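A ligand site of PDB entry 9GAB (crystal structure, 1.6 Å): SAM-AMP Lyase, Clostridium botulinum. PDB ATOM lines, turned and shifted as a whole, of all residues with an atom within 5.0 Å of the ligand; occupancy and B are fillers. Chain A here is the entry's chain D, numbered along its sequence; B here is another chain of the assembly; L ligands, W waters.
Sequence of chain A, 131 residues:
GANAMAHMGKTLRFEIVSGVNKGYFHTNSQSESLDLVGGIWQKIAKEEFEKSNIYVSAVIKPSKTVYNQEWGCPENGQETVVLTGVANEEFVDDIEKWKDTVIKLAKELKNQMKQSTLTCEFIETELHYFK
An oxygen (O6) of the ligand is in hydrogen-bond range of the side-chain hydroxyl of Thr 117 of chain B (2.7 Å). The side-chain hydroxyl (OG1) of Thr 119 of chain B is in hydrogen-bond range of a nitrogen (N5) of the ligand. An oxygen (O5) of the ligand is in hydrogen-bond range of the side-chain hydroxyl of Tyr 129, 2.5 Å away. O of Tyr 55 lies within hydrogen-bond range of N10 of the ligand (3.2 Å). The side-chain hydroxyl (OG) of Ser 57 sits at hydrogen-bond distance from a nitrogen (N1) of the ligand (2.6 Å).
The backbone carbonyl oxygen (O) of Gln 78 of chain B is in hydrogen-bond range of the backbone NH (N) of Thr 65 of chain B, 2.8 Å away. O of Tyr 67 of chain B lies close to OH of Tyr 55 (3.4 Å). The backbone NH (N) of Val 59 lies within hydrogen-bond range of the backbone carbonyl oxygen (O) of Thr 84. The side-chain amide oxygen (OE1) of Gln 78 of chain B is in hydrogen-bond range of the side-chain hydroxyl (OH) of Tyr 67 of chain B. The side-chain hydroxyl (OG1) of Thr 65 of chain B lies within hydrogen-bond range of the side-chain hydroxyl (OG1) of Thr 80 of chain B, 2.8 Å away. The backbone NH (N) of Val 17 of chain B lies within hydrogen-bond range of the backbone carbonyl oxygen (O) of Thr 119 of chain B, 3.3 Å away.
Merely in contact with the ligand: Val 59 (3.8 Å), Gly 85 (3.7 Å), Val 86 (3.8 Å), Phe 91 (3.5 Å), Val 17 of chain B (3.5 Å), Thr 65 of chain B (3.4 Å), Tyr 67 of chain B (3.5 Å), Trp 71 of chain B (3.2 Å) and Gln 78 of chain B (3.8 Å). 14 residues have an atom within 4 Å of the ligand: Tyr 55, Ser 57, Val 59, Gly 85, Val 86, Phe 91, Tyr 129, Val 17 of chain B, Thr 65 of chain B, Tyr 67 of chain B, Trp 71 of chain B, Gln 78 of chain B, Thr 117 of chain B and Thr 119 of chain B. Along chain A the residues within 4 Å of the ligand span positions 55 to 129.
Water W4 bridges N9 of the ligand and N of Tyr 55. Water W8 bridges an oxygen (O8) of the ligand (2.7 Å) and the side-chain hydroxyl of Tyr 129 (2.8 Å). Water W2 bridges a nitrogen (N10) of the ligand (2.8 Å) and the side-chain hydroxyl of Ser 57 (3.0 Å). Water W3 lies within hydrogen-bond range of O of Val 17 of chain B, N3 of the ligand and N of Thr 119 of chain B.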
ATOM      1  N   TYR A  55      -3.556 -12.067 -12.997  1.00  0.00           N
ATOM      2  CA  TYR A  55      -2.676 -13.188 -13.232  1.00  0.00           C
ATOM      3  C   TYR A  55      -2.897 -14.235 -12.136  1.00  0.00           C
ATOM      4  O   TYR A  55      -2.703 -13.933 -10.959  1.00  0.00           O
ATOM      5  CB  TYR A  55      -1.191 -12.797 -13.215  1.00  0.00           C
ATOM      6  CG  TYR A  55      -0.314 -13.912 -13.757  1.00  0.00           C
ATOM      7  CD1 TYR A  55       0.011 -14.996 -12.964  1.00  0.00           C
ATOM      8  CD2 TYR A  55       0.150 -13.934 -15.067  1.00  0.00           C
ATOM      9  CE1 TYR A  55       0.730 -16.067 -13.457  1.00  0.00           C
ATOM     10  CE2 TYR A  55       0.888 -14.992 -15.579  1.00  0.00           C
ATOM     11  CZ  TYR A  55       1.189 -16.064 -14.749  1.00  0.00           C
ATOM     12  OH  TYR A  55       1.920 -17.124 -15.212  1.00  0.00           O
ATOM     13  N   SER A  57      -1.314 -17.301 -10.588  1.00  0.00           N
ATOM     14  CA  SER A  57      -0.186 -18.212 -10.419  1.00  0.00           C
ATOM     15  C   SER A  57      -0.646 -19.513  -9.773  1.00  0.00           C
ATOM     16  O   SER A  57      -1.644 -19.548  -9.051  1.00  0.00           O
ATOM     17  CB  SER A  57       0.902 -17.547  -9.596  1.00  0.00           C
ATOM     18  OG  SER A  57       0.468 -17.208  -8.287  1.00  0.00           O
ATOM     19  N   ALA A  58       0.072 -20.611 -10.061  1.00  0.00           N
ATOM     20  CA  ALA A  58      -0.298 -21.926  -9.554  1.00  0.00           C
ATOM     21  C   ALA A  58       0.922 -22.734  -9.118  1.00  0.00           C
ATOM     22  O   ALA A  58       1.951 -22.779  -9.790  1.00  0.00           O
ATOM     23  CB  ALA A  58      -1.054 -22.657 -10.624  1.00  0.00           C
ATOM     24  N   VAL A  59       0.770 -23.404  -7.976  1.00  0.00           N
ATOM     25  CA  VAL A  59       1.729 -24.387  -7.491  1.00  0.00           C
ATOM     26  C   VAL A  59       1.242 -25.756  -7.974  1.00  0.00           C
ATOM     27  O   VAL A  59       0.097 -26.142  -7.688  1.00  0.00           O
ATOM     28  CB  VAL A  59       1.804 -24.339  -5.952  1.00  0.00           C
ATOM     29  CG1 VAL A  59       2.819 -25.322  -5.403  1.00  0.00           C
ATOM     30  CG2 VAL A  59       2.104 -22.928  -5.442  1.00  0.00           C
ATOM     31  N   THR A  84      -2.687 -25.547  -7.176  1.00  0.00           N
ATOM     32  CA  THR A  84      -3.262 -24.739  -6.115  1.00  0.00           C
ATOM     33  C   THR A  84      -2.764 -23.293  -6.203  1.00  0.00           C
ATOM     34  O   THR A  84      -1.674 -23.036  -6.695  1.00  0.00           O
ATOM     35  CB  THR A  84      -2.912 -25.331  -4.750  1.00  0.00           C
ATOM     36  OG1 THR A  84      -1.511 -25.164  -4.518  1.00  0.00           O
ATOM     37  CG2 THR A  84      -3.250 -26.806  -4.638  1.00  0.00           C
ATOM     38  N   GLY A  85      -3.557 -22.346  -5.710  1.00  0.00           N
ATOM     39  CA  GLY A  85      -3.101 -20.969  -5.628  1.00  0.00           C
ATOM     40  C   GLY A  85      -3.953 -20.153  -4.696  1.00  0.00           C
ATOM     41  O   GLY A  85      -4.977 -20.638  -4.230  1.00  0.00           O
ATOM     42  N   VAL A  86      -3.491 -18.959  -4.323  1.00  0.00           N
ATOM     43  CA  VAL A  86      -4.212 -18.115  -3.370  1.00  0.00           C
ATOM     44  C   VAL A  86      -4.409 -16.729  -3.981  1.00  0.00           C
ATOM     45  O   VAL A  86      -3.578 -16.272  -4.742  1.00  0.00           O
ATOM     46  CB  VAL A  86      -3.393 -18.092  -2.074  1.00  0.00           C
ATOM     47  CG1 VAL A  86      -2.019 -17.476  -2.274  1.00  0.00           C
ATOM     48  CG2 VAL A  86      -4.104 -17.360  -0.930  1.00  0.00           C
ATOM     49  N   PHE A  91      -1.955  -8.340  -5.087  1.00  0.00           N
ATOM     50  CA  PHE A  91      -2.147  -8.371  -6.531  1.00  0.00           C
ATOM     51  C   PHE A  91      -3.623  -8.399  -6.935  1.00  0.00           C
ATOM     52  O   PHE A  91      -3.920  -8.153  -8.111  1.00  0.00           O
ATOM     53  CB  PHE A  91      -1.499  -9.617  -7.136  1.00  0.00           C
ATOM     54  CG  PHE A  91      -0.068  -9.862  -6.708  1.00  0.00           C
ATOM     55  CD1 PHE A  91       0.895  -8.863  -6.818  1.00  0.00           C
ATOM     56  CD2 PHE A  91       0.308 -11.086  -6.163  1.00  0.00           C
ATOM     57  CE1 PHE A  91       2.205  -9.090  -6.403  1.00  0.00           C
ATOM     58  CE2 PHE A  91       1.608 -11.317  -5.750  1.00  0.00           C
ATOM     59  CZ  PHE A  91       2.553 -10.322  -5.871  1.00  0.00           C
ATOM     60  N   TYR A 129       1.678 -12.901   3.997  1.00  0.00           N
ATOM     61  CA  TYR A 129       2.612 -12.683   2.920  1.00  0.00           C
ATOM     62  C   TYR A 129       3.801 -11.864   3.449  1.00  0.00           C
ATOM     63  O   TYR A 129       3.600 -10.751   3.925  1.00  0.00           O
ATOM     64  CB  TYR A 129       1.896 -11.973   1.783  1.00  0.00           C
ATOM     65  CG  TYR A 129       2.723 -11.686   0.539  1.00  0.00           C
ATOM     66  CD1 TYR A 129       3.453 -12.678  -0.110  1.00  0.00           C
ATOM     67  CD2 TYR A 129       2.752 -10.403  -0.013  1.00  0.00           C
ATOM     68  CE1 TYR A 129       4.159 -12.404  -1.278  1.00  0.00           C
ATOM     69  CE2 TYR A 129       3.430 -10.138  -1.195  1.00  0.00           C
ATOM     70  CZ  TYR A 129       4.160 -11.139  -1.814  1.00  0.00           C
ATOM     71  OH  TYR A 129       4.854 -10.852  -2.958  1.00  0.00           O
ATOM     72  N   VAL B  17       4.782 -22.151   1.030  1.00  0.00           N
ATOM     73  CA  VAL B  17       5.426 -22.422  -0.244  1.00  0.00           C
ATOM     74  C   VAL B  17       6.751 -21.658  -0.291  1.00  0.00           C
ATOM     75  O   VAL B  17       6.774 -20.441  -0.019  1.00  0.00           O
ATOM     76  CB  VAL B  17       4.504 -22.015  -1.398  1.00  0.00           C
ATOM     77  CG1 VAL B  17       5.150 -22.306  -2.750  1.00  0.00           C
ATOM     78  CG2 VAL B  17       3.158 -22.728  -1.323  1.00  0.00           C
ATOM     79  N   GLY B  19      10.669 -21.251  -2.561  1.00  0.00           N
ATOM     80  CA  GLY B  19      11.717 -21.572  -3.536  1.00  0.00           C
ATOM     81  C   GLY B  19      12.880 -22.318  -2.906  1.00  0.00           C
ATOM     82  O   GLY B  19      12.926 -22.500  -1.676  1.00  0.00           O
ATOM     83  N   THR B  65       6.200 -23.977  -9.302  1.00  0.00           N
ATOM     84  CA  THR B  65       5.262 -22.864  -9.224  1.00  0.00           C
ATOM     85  C   THR B  65       5.366 -22.030 -10.512  1.00  0.00           C
ATOM     86  O   THR B  65       6.466 -21.648 -10.916  1.00  0.00           O
ATOM     87  CB  THR B  65       5.582 -22.036  -7.992  1.00  0.00           C
ATOM     88  OG1 THR B  65       5.369 -22.877  -6.837  1.00  0.00           O
ATOM     89  CG2 THR B  65       4.665 -20.852  -7.792  1.00  0.00           C
ATOM     90  N   TYR B  67       4.426 -18.756 -12.767  1.00  0.00           N
ATOM     91  CA  TYR B  67       4.050 -17.363 -12.866  1.00  0.00           C
ATOM     92  C   TYR B  67       4.723 -16.778 -14.116  1.00  0.00           C
ATOM     93  O   TYR B  67       5.322 -17.503 -14.924  1.00  0.00           O
ATOM     94  CB  TYR B  67       4.358 -16.629 -11.550  1.00  0.00           C
ATOM     95  CG  TYR B  67       5.823 -16.662 -11.100  1.00  0.00           C
ATOM     96  CD1 TYR B  67       6.400 -17.817 -10.543  1.00  0.00           C
ATOM     97  CD2 TYR B  67       6.616 -15.525 -11.178  1.00  0.00           C
ATOM     98  CE1 TYR B  67       7.739 -17.846 -10.166  1.00  0.00           C
ATOM     99  CE2 TYR B  67       7.937 -15.544 -10.791  1.00  0.00           C
ATOM    100  CZ  TYR B  67       8.506 -16.694 -10.266  1.00  0.00           C
ATOM    101  OH  TYR B  67       9.828 -16.719  -9.871  1.00  0.00           O
ATOM    102  N   TRP B  71       8.516 -11.821 -14.712  1.00  0.00           N
ATOM    103  CA  TRP B  71       8.807 -11.566 -13.313  1.00  0.00           C
ATOM    104  C   TRP B  71       9.885 -12.502 -12.805  1.00  0.00           C
ATOM    105  O   TRP B  71      10.153 -12.532 -11.594  1.00  0.00           O
ATOM    106  CB  TRP B  71       7.518 -11.680 -12.470  1.00  0.00           C
ATOM    107  CG  TRP B  71       6.357 -10.866 -12.988  1.00  0.00           C
ATOM    108  CD1 TRP B  71       6.428  -9.669 -13.648  1.00  0.00           C
ATOM    109  CD2 TRP B  71       4.950 -11.189 -12.883  1.00  0.00           C
ATOM    110  NE1 TRP B  71       5.173  -9.243 -13.992  1.00  0.00           N
ATOM    111  CE2 TRP B  71       4.243 -10.146 -13.533  1.00  0.00           C
ATOM    112  CE3 TRP B  71       4.233 -12.249 -12.328  1.00  0.00           C
ATOM    113  CZ2 TRP B  71       2.852 -10.140 -13.630  1.00  0.00           C
ATOM    114  CZ3 TRP B  71       2.850 -12.238 -12.423  1.00  0.00           C
ATOM    115  CH2 TRP B  71       2.171 -11.206 -13.073  1.00  0.00           C
ATOM    116  N   GLN B  78       9.000 -22.599 -11.662  1.00  0.00           N
ATOM    117  CA  GLN B  78      10.116 -22.577 -10.721  1.00  0.00           C
ATOM    118  C   GLN B  78      10.022 -23.771  -9.768  1.00  0.00           C
ATOM    119  O   GLN B  78       8.971 -24.056  -9.229  1.00  0.00           O
ATOM    120  CB  GLN B  78      10.039 -21.272  -9.919  1.00  0.00           C
ATOM    121  CG  GLN B  78      11.171 -21.104  -8.926  1.00  0.00           C
ATOM    122  CD  GLN B  78      11.061 -19.862  -8.075  1.00  0.00           C
ATOM    123  OE1 GLN B  78      10.366 -18.909  -8.419  1.00  0.00           O
ATOM    124  NE2 GLN B  78      11.783 -19.803  -6.972  1.00  0.00           N
ATOM    125  N   THR B  80       9.914 -25.605  -6.482  1.00  0.00           N
ATOM    126  CA  THR B  80       9.456 -25.156  -5.165  1.00  0.00           C
ATOM    127  C   THR B  80       9.195 -26.380  -4.277  1.00  0.00           C
ATOM    128  O   THR B  80       9.171 -27.517  -4.766  1.00  0.00           O
ATOM    129  CB  THR B  80       8.214 -24.267  -5.279  1.00  0.00           C
ATOM    130  OG1 THR B  80       7.248 -24.836  -6.167  1.00  0.00           O
ATOM    131  CG2 THR B  80       8.530 -22.856  -5.768  1.00  0.00           C
ATOM    132  N   THR B 117      10.423 -13.503  -1.083  1.00  0.00           N
ATOM    133  CA  THR B 117       9.031 -13.517  -0.634  1.00  0.00           C
ATOM    134  C   THR B 117       8.666 -14.926  -0.133  1.00  0.00           C
ATOM    135  O   THR B 117       9.335 -15.903  -0.499  1.00  0.00           O
ATOM    136  CB  THR B 117       8.030 -13.112  -1.725  1.00  0.00           C
ATOM    137  OG1 THR B 117       8.010 -14.136  -2.731  1.00  0.00           O
ATOM    138  CG2 THR B 117       8.346 -11.759  -2.356  1.00  0.00           C
ATOM    139  N   THR B 119       4.858 -17.231   1.275  1.00  0.00           N
ATOM    140  CA  THR B 119       3.462 -17.344   1.717  1.00  0.00           C
ATOM    141  C   THR B 119       3.338 -18.351   2.860  1.00  0.00           C
ATOM    142  O   THR B 119       3.940 -19.440   2.799  1.00  0.00           O
ATOM    143  CB  THR B 119       2.511 -17.743   0.586  1.00  0.00           C
ATOM    144  OG1 THR B 119       2.879 -19.009   0.006  1.00  0.00           O
ATOM    145  CG2 THR B 119       2.468 -16.746  -0.558  1.00  0.00           C
ATOM    146  N   GLU B 121      -0.172 -19.830   4.893  1.00  0.00           N
ATOM    147  CA  GLU B 121      -1.625 -19.822   5.058  1.00  0.00           C
ATOM    148  C   GLU B 121      -2.046 -20.622   6.294  1.00  0.00           C
ATOM    149  O   GLU B 121      -1.408 -21.608   6.612  1.00  0.00           O
ATOM    150  CB  GLU B 121      -2.264 -20.436   3.839  1.00  0.00           C
ATOM    151  CG  GLU B 121      -2.233 -19.548   2.604  1.00  0.00           C
ATOM    152  CD  GLU B 121      -2.589 -20.358   1.391  1.00  0.00           C
ATOM    153  OE1 GLU B 121      -3.780 -20.760   1.362  1.00  0.00           O
ATOM    154  OE2 GLU B 121      -1.697 -20.673   0.562  1.00  0.00           O
HETATM  155  C1  LIG L   1       2.427 -18.965  -4.162  1.00  0.00           C
HETATM  156  C2  LIG L   1       2.385 -18.523  -5.468  1.00  0.00           C
HETATM  157  N1  LIG L   1       1.397 -18.744  -6.351  1.00  0.00           N
HETATM  158  C3  LIG L   1       0.358 -19.333  -5.758  1.00  0.00           C
HETATM  159  N2  LIG L   1       0.239 -19.798  -4.501  1.00  0.00           N
HETATM  160  C4  LIG L   1       1.282 -19.582  -3.656  1.00  0.00           C
HETATM  161  N3  LIG L   1       3.653 -18.642  -3.611  1.00  0.00           N
HETATM  162  N4  LIG L   1       3.627 -17.988  -5.714  1.00  0.00           N
HETATM  163  C5  LIG L   1       4.322 -18.063  -4.578  1.00  0.00           C
HETATM  164  N5  LIG L   1       1.176 -19.990  -2.386  1.00  0.00           N
HETATM  165  C6  LIG L   1       4.068 -17.350  -6.969  1.00  0.00           C
HETATM  166  O1  LIG L   1       5.460 -17.594  -7.131  1.00  0.00           O
HETATM  167  C7  LIG L   1       6.172 -16.339  -7.222  1.00  0.00           C
HETATM  168  C8  LIG L   1       5.288 -15.355  -6.462  1.00  0.00           C
HETATM  169  C9  LIG L   1       3.904 -15.833  -6.958  1.00  0.00           C
HETATM  170  O2  LIG L   1       3.604 -15.340  -8.253  1.00  0.00           O
HETATM  171  O3  LIG L   1       5.601 -14.003  -6.831  1.00  0.00           O
HETATM  172  P1  LIG L   1       6.168 -13.011  -5.664  1.00  0.00           P
HETATM  173  O4  LIG L   1       6.099 -11.661  -6.549  1.00  0.00           O
HETATM  174  O5  LIG L   1       5.149 -12.755  -4.605  1.00  0.00           O
HETATM  175  O6  LIG L   1       7.551 -13.445  -5.312  1.00  0.00           O
HETATM  176  S1  LIG L   1       7.844 -17.099  -5.066  1.00  0.00           S
HETATM  177  C10 LIG L   1       7.618 -16.474  -6.754  1.00  0.00           C
HETATM  178  C11 LIG L   1       8.037 -18.843  -5.396  1.00  0.00           C
HETATM  179  C12 LIG L   1       7.289 -11.085  -7.180  1.00  0.00           C
HETATM  180  C13 LIG L   1       6.860  -9.955  -8.093  1.00  0.00           C
HETATM  181  C14 LIG L   1       5.770  -9.029  -7.535  1.00  0.00           C
HETATM  182  C15 LIG L   1       5.139  -8.519  -8.820  1.00  0.00           C
HETATM  183  C16 LIG L   1       5.101  -9.819  -9.635  1.00  0.00           C
HETATM  184  O7  LIG L   1       6.290 -10.504  -9.316  1.00  0.00           O
HETATM  185  O8  LIG L   1       6.365  -8.042  -6.688  1.00  0.00           O
HETATM  186  O9  LIG L   1       5.966  -7.567  -9.473  1.00  0.00           O
HETATM  187  N6  LIG L   1       3.974 -10.723  -9.402  1.00  0.00           N
HETATM  188  C17 LIG L   1       2.647 -10.488  -9.682  1.00  0.00           C
HETATM  189  C18 LIG L   1       1.977 -11.659  -9.378  1.00  0.00           C
HETATM  190  N7  LIG L   1       2.853 -12.605  -8.863  1.00  0.00           N
HETATM  191  C19 LIG L   1       4.021 -12.003  -8.898  1.00  0.00           C
HETATM  192  N8  LIG L   1       2.101  -9.384 -10.207  1.00  0.00           N
HETATM  193  C20 LIG L   1       0.793  -9.528 -10.390  1.00  0.00           C
HETATM  194  N9  LIG L   1      -0.003 -10.576 -10.122  1.00  0.00           N
HETATM  195  C21 LIG L   1       0.592 -11.701  -9.622  1.00  0.00           C
HETATM  196  N10 LIG L   1      -0.183 -12.751  -9.335  1.00  0.00           N
HETATM  197  O   HOH W   1       3.592 -14.901  -3.564  1.00  0.00           O
HETATM  198  O   HOH W   2       0.311 -14.463  -7.158  1.00  0.00           O
HETATM  199  O   HOH W   3       5.778 -18.598  -1.535  1.00  0.00           O
HETATM  200  O   HOH W   4      -2.438 -10.179 -11.101  1.00  0.00           O
HETATM  201  O   HOH W   5      10.007 -13.341  -5.833  1.00  0.00           O
HETATM  202  O   HOH W   6       8.561  -6.576  -7.353  1.00  0.00           O
HETATM  203  O   HOH W   7       2.898  -7.061 -11.526  1.00  0.00           O
HETATM  204  O   HOH W   8       5.961  -8.539  -4.069  1.00  0.00           O
